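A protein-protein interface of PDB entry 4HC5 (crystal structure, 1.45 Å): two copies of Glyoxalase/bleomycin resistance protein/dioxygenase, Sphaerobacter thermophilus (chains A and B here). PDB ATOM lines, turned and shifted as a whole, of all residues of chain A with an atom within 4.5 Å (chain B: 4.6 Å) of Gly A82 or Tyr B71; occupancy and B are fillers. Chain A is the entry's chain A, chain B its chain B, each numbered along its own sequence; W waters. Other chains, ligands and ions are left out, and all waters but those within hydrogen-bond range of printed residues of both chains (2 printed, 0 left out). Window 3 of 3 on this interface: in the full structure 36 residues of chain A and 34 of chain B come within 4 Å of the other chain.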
ATOM      1  N   TYR A  80     -22.273 -14.768  14.389  1.00  0.00           N
ATOM      2  CA  TYR A  80     -23.386 -13.949  13.916  1.00  0.00           C
ATOM      3  C   TYR A  80     -24.186 -13.381  15.032  1.00  0.00           C
ATOM      4  O   TYR A  80     -24.645 -14.101  15.832  1.00  0.00           O
ATOM      5  CB  TYR A  80     -24.315 -14.781  13.050  1.00  0.00           C
ATOM      6  CG  TYR A  80     -23.646 -15.150  11.824  1.00  0.00           C
ATOM      7  CD1 TYR A  80     -23.315 -14.199  10.888  1.00  0.00           C
ATOM      8  CD2 TYR A  80     -23.274 -16.462  11.601  1.00  0.00           C
ATOM      9  CE1 TYR A  80     -22.651 -14.551   9.735  1.00  0.00           C
ATOM     10  CE2 TYR A  80     -22.619 -16.826  10.451  1.00  0.00           C
ATOM     11  CZ  TYR A  80     -22.306 -15.865   9.537  1.00  0.00           C
ATOM     12  OH  TYR A  80     -21.662 -16.249   8.421  1.00  0.00           O
ATOM     13  N   THR A  81     -24.331 -12.068  15.066  1.00  0.00           N
ATOM     14  CA  THR A  81     -25.090 -11.426  16.114  1.00  0.00           C
ATOM     15  C   THR A  81     -26.578 -11.416  15.818  1.00  0.00           C
ATOM     16  O   THR A  81     -27.345 -11.250  16.693  1.00  0.00           O
ATOM     17  CB  THR A  81     -24.680  -9.968  16.314  1.00  0.00           C
ATOM     18  OG1 THR A  81     -24.865  -9.246  15.109  1.00  0.00           O
ATOM     19  CG2 THR A  81     -23.238  -9.854  16.767  1.00  0.00           C
ATOM     20  N   GLY A  82     -26.913 -11.556  14.560  1.00  0.00           N
ATOM     21  CA  GLY A  82     -28.329 -11.366  14.143  1.00  0.00           C
ATOM     22  C   GLY A  82     -28.686  -9.892  14.087  1.00  0.00           C
ATOM     23  O   GLY A  82     -29.838  -9.524  13.901  1.00  0.00           O
ATOM     24  N   ILE A  83     -27.715  -9.005  14.272  1.00  0.00           N
ATOM     25  CA  ILE A  83     -27.917  -7.524  14.216  1.00  0.00           C
ATOM     26  C   ILE A  83     -27.475  -7.046  12.848  1.00  0.00           C
ATOM     27  O   ILE A  83     -26.357  -7.273  12.388  1.00  0.00           O
ATOM     28  CB  ILE A  83     -27.203  -6.772  15.338  1.00  0.00           C
ATOM     29  CG1 ILE A  83     -27.799  -7.164  16.686  1.00  0.00           C
ATOM     30  CG2 ILE A  83     -27.282  -5.244  15.150  1.00  0.00           C
ATOM     31  CD1 ILE A  83     -27.009  -6.731  17.930  1.00  0.00           C
ATOM     32  N   SER A  84     -28.383  -6.294  12.219  1.00  0.00           N
ATOM     33  CA  SER A  84     -28.087  -5.637  10.949  1.00  0.00           C
ATOM     34  C   SER A  84     -28.064  -4.130  11.212  1.00  0.00           C
ATOM     35  O   SER A  84     -28.876  -3.586  11.986  1.00  0.00           O
ATOM     36  CB  SER A  84     -29.096  -5.951   9.878  1.00  0.00           C
ATOM     37  OG  SER A  84     -29.160  -7.348   9.603  1.00  0.00           O
ATOM     38  N   SER B  16     -32.325  -4.028  12.746  1.00  0.00           N
ATOM     39  CA  SER B  16     -33.021  -5.135  13.330  1.00  0.00           C
ATOM     40  C   SER B  16     -32.086  -5.976  14.175  1.00  0.00           C
ATOM     41  O   SER B  16     -30.898  -6.027  13.957  1.00  0.00           O
ATOM     42  CB  SER B  16     -33.678  -6.046  12.278  1.00  0.00           C
ATOM     43  OG  SER B  16     -32.793  -6.415  11.254  1.00  0.00           O
ATOM     44  N   ALA B  17     -32.717  -6.647  15.134  1.00  0.00           N
ATOM     45  CA  ALA B  17     -32.138  -7.750  15.915  1.00  0.00           C
ATOM     46  C   ALA B  17     -32.969  -8.972  15.697  1.00  0.00           C
ATOM     47  O   ALA B  17     -34.104  -8.877  15.282  1.00  0.00           O
ATOM     48  CB  ALA B  17     -32.072  -7.363  17.420  1.00  0.00           C
ATOM     49  N   THR B  18     -32.393 -10.139  15.965  1.00  0.00           N
ATOM     50  CA  THR B  18     -33.007 -11.423  15.644  1.00  0.00           C
ATOM     51  C   THR B  18     -33.337 -12.202  16.888  1.00  0.00           C
ATOM     52  O   THR B  18     -32.537 -12.276  17.795  1.00  0.00           O
ATOM     53  CB  THR B  18     -32.112 -12.247  14.680  1.00  0.00           C
ATOM     54  OG1 THR B  18     -31.820 -11.434  13.535  1.00  0.00           O
ATOM     55  CG2 THR B  18     -32.779 -13.554  14.246  1.00  0.00           C
ATOM     56  N   ILE B  20     -34.967 -16.257  17.910  1.00  0.00           N
ATOM     57  CA  ILE B  20     -35.178 -17.604  17.341  1.00  0.00           C
ATOM     58  C   ILE B  20     -36.519 -18.115  17.797  1.00  0.00           C
ATOM     59  O   ILE B  20     -36.769 -18.197  19.012  1.00  0.00           O
ATOM     60  CB  ILE B  20     -34.062 -18.573  17.750  1.00  0.00           C
ATOM     61  CG1 ILE B  20     -32.715 -17.923  17.407  1.00  0.00           C
ATOM     62  CG2 ILE B  20     -34.252 -19.936  17.098  1.00  0.00           C
ATOM     63  CD1 ILE B  20     -32.458 -17.595  15.970  1.00  0.00           C
ATOM     64  N   LEU B  67     -35.316 -18.715  12.572  1.00  0.00           N
ATOM     65  CA  LEU B  67     -35.487 -20.106  12.894  1.00  0.00           C
ATOM     66  C   LEU B  67     -34.081 -20.680  13.236  1.00  0.00           C
ATOM     67  O   LEU B  67     -33.089 -20.204  12.726  1.00  0.00           O
ATOM     68  CB  LEU B  67     -36.090 -20.835  11.704  1.00  0.00           C
ATOM     69  CG  LEU B  67     -37.551 -20.587  11.343  1.00  0.00           C
ATOM     70  CD1 LEU B  67     -37.859 -21.318  10.002  1.00  0.00           C
ATOM     71  CD2 LEU B  67     -38.506 -21.108  12.413  1.00  0.00           C
ATOM     72  N   PRO B  68     -34.073 -21.823  13.939  1.00  0.00           N
ATOM     73  CA  PRO B  68     -32.822 -22.535  14.146  1.00  0.00           C
ATOM     74  C   PRO B  68     -32.104 -22.854  12.856  1.00  0.00           C
ATOM     75  O   PRO B  68     -30.874 -22.757  12.818  1.00  0.00           O
ATOM     76  CB  PRO B  68     -33.275 -23.772  14.884  1.00  0.00           C
ATOM     77  CG  PRO B  68     -34.510 -23.376  15.657  1.00  0.00           C
ATOM     78  CD  PRO B  68     -35.204 -22.429  14.695  1.00  0.00           C
ATOM     79  N   SER B  69     -32.868 -23.075  11.789  1.00  0.00           N
ATOM     80  CA  SER B  69     -32.325 -23.451  10.446  1.00  0.00           C
ATOM     81  C   SER B  69     -31.561 -22.317   9.816  1.00  0.00           C
ATOM     82  O   SER B  69     -30.803 -22.524   8.892  1.00  0.00           O
ATOM     83  CB  SER B  69     -33.428 -23.974   9.550  1.00  0.00           C
ATOM     84  OG  SER B  69     -34.320 -22.937   9.279  1.00  0.00           O
ATOM     85  N   TRP B  70     -31.750 -21.116  10.335  1.00  0.00           N
ATOM     86  CA  TRP B  70     -31.013 -19.971   9.801  1.00  0.00           C
ATOM     87  C   TRP B  70     -29.541 -20.031  10.123  1.00  0.00           C
ATOM     88  O   TRP B  70     -28.764 -19.320   9.570  1.00  0.00           O
ATOM     89  CB  TRP B  70     -31.527 -18.645  10.335  1.00  0.00           C
ATOM     90  CG  TRP B  70     -32.841 -18.195   9.798  1.00  0.00           C
ATOM     91  CD1 TRP B  70     -33.772 -18.909   9.126  1.00  0.00           C
ATOM     92  CD2 TRP B  70     -33.360 -16.860   9.931  1.00  0.00           C
ATOM     93  NE1 TRP B  70     -34.827 -18.093   8.791  1.00  0.00           N
ATOM     94  CE2 TRP B  70     -34.629 -16.853   9.282  1.00  0.00           C
ATOM     95  CE3 TRP B  70     -32.875 -15.678  10.494  1.00  0.00           C
ATOM     96  CZ2 TRP B  70     -35.398 -15.666   9.164  1.00  0.00           C
ATOM     97  CZ3 TRP B  70     -33.676 -14.522  10.428  1.00  0.00           C
ATOM     98  CH2 TRP B  70     -34.922 -14.539   9.743  1.00  0.00           C
ATOM     99  N   TYR B  71     -29.201 -20.824  11.146  1.00  0.00           N
ATOM    100  CA  TYR B  71     -27.863 -20.871  11.772  1.00  0.00           C
ATOM    101  C   TYR B  71     -27.258 -22.271  11.809  1.00  0.00           C
ATOM    102  O   TYR B  71     -27.947 -23.239  11.795  1.00  0.00           O
ATOM    103  CB  TYR B  71     -27.931 -20.257  13.196  1.00  0.00           C
ATOM    104  CG  TYR B  71     -28.372 -18.824  13.124  1.00  0.00           C
ATOM    105  CD1 TYR B  71     -27.438 -17.828  12.837  1.00  0.00           C
ATOM    106  CD2 TYR B  71     -29.725 -18.427  13.313  1.00  0.00           C
ATOM    107  CE1 TYR B  71     -27.799 -16.477  12.733  1.00  0.00           C
ATOM    108  CE2 TYR B  71     -30.080 -17.079  13.200  1.00  0.00           C
ATOM    109  CZ  TYR B  71     -29.120 -16.082  12.916  1.00  0.00           C
ATOM    110  OH  TYR B  71     -29.395 -14.693  12.811  1.00  0.00           O
ATOM    111  N   GLU B  72     -25.963 -22.361  11.887  1.00  0.00           N
ATOM    112  CA  GLU B  72     -25.260 -23.654  11.924  1.00  0.00           C
ATOM    113  C   GLU B  72     -24.705 -23.980  13.324  1.00  0.00           C
ATOM    114  O   GLU B  72     -24.093 -24.986  13.581  1.00  0.00           O
ATOM    115  CB  GLU B  72     -24.113 -23.581  10.921  1.00  0.00           C
ATOM    116  N   ASP B  73     -24.933 -23.086  14.242  1.00  0.00           N
ATOM    117  CA  ASP B  73     -24.352 -23.235  15.605  1.00  0.00           C
ATOM    118  C   ASP B  73     -25.223 -23.825  16.687  1.00  0.00           C
ATOM    119  O   ASP B  73     -24.864 -23.767  17.857  1.00  0.00           O
ATOM    120  CB  ASP B  73     -23.770 -21.921  16.130  1.00  0.00           C
ATOM    121  CG  ASP B  73     -24.830 -20.955  16.561  1.00  0.00           C
ATOM    122  OD1 ASP B  73     -26.032 -21.115  16.212  1.00  0.00           O
ATOM    123  OD2 ASP B  73     -24.453 -20.010  17.272  1.00  0.00           O
ATOM    124  N   ARG B  75     -28.281 -22.889  17.694  1.00  0.00           N
ATOM    125  CA  ARG B  75     -29.121 -21.968  18.489  1.00  0.00           C
ATOM    126  C   ARG B  75     -30.618 -22.327  18.347  1.00  0.00           C
ATOM    127  O   ARG B  75     -31.141 -22.603  17.319  1.00  0.00           O
ATOM    128  CB  ARG B  75     -28.857 -20.522  18.211  1.00  0.00           C
ATOM    129  CG  ARG B  75     -29.323 -19.977  16.893  1.00  0.00           C
ATOM    130  CD  ARG B  75     -28.826 -18.527  16.682  1.00  0.00           C
ATOM    131  NE  ARG B  75     -27.380 -18.428  16.589  1.00  0.00           N
ATOM    132  CZ  ARG B  75     -26.730 -17.262  16.409  1.00  0.00           C
ATOM    133  NH1 ARG B  75     -27.388 -16.108  16.382  1.00  0.00           N
ATOM    134  NH2 ARG B  75     -25.397 -17.230  16.281  1.00  0.00           N
HETATM  135  O   HOH W   1     -30.976  -8.422  11.459  1.00  0.00           O
HETATM  136  O   HOH W   2     -29.871 -10.299  17.324  1.00  0.00           O
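N of Ile A83 sits at hydrogen-bond distance from OG1 of Thr A81 (3.0 Å). NE of Arg B75 lies within salt-bridge range of OD1 of Asp B73 (3.0 Å).
Among the printed residues, pairs that only touch across the chains: Ile A83 with Ser B16, Gly A82 with Ala B17, Gly A82 with Ser B16, Gly A82 with Tyr B71 and Tyr A80 with Tyr B71.
Of chain B, only Ser B16, Ala B17, Thr B18 and Tyr B71 come within 4 Å of Gly A82. Printed residues of chain A within 4 Å of Tyr B71: Tyr A80 and Gly A82. Printed residues of chain A within 4 Å of Ser B16: Gly A82 (3.7 Å), Ile A83 (3.3 Å) and Ser A84 (3.1 Å). Of the printed residues of chain B, Tyr A80 touches Tyr B71 (3.9 Å) and Arg B75 (3.2 Å). Printed residues of chain A within 4 Å of Arg B75: Tyr A80. Of the printed residues of chain B, Ser A84 touches Ser B16 (3.1 Å). Of the printed residues of chain A, Ala B17 touches Gly A82. The nearest printed residue of chain B that does not touch Gly A82 is Arg B75 (4.9 Å). The nearest printed residue of chain A that does not touch Tyr B71 is Thr A81 (5.3 Å). The nearest printed residue of chain B that does not touch Tyr A80 is Asp B73 (6.1 Å).
Water W1 lies within hydrogen-bond range of the side-chain hydroxyl of Ser B16, the side-chain hydroxyl of Ser A84 and the backbone carbonyl oxygen of Gly A82. Water W2 bridges O of Thr A81 and N of Thr B18.
No position is printed for both chains.
Hydrophobic or aromatic side chains of chain A that line the printed part of chain B: Tyr A80 and Ile A83. Hydrophobic or aromatic side chains of chain B within 4 Å of the printed part of chain A: Tyr B71.
The backbone carbonyl oxygen (O) of Tyr A80 is in hydrogen-bond range of the guanidinium group (NH2) of Arg B75, at 3.2 Å. N of Ser A84 is in hydrogen-bond range of O of Ser B16. OG1 of Thr B18 sits at hydrogen-bond distance from O of Gly A82.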
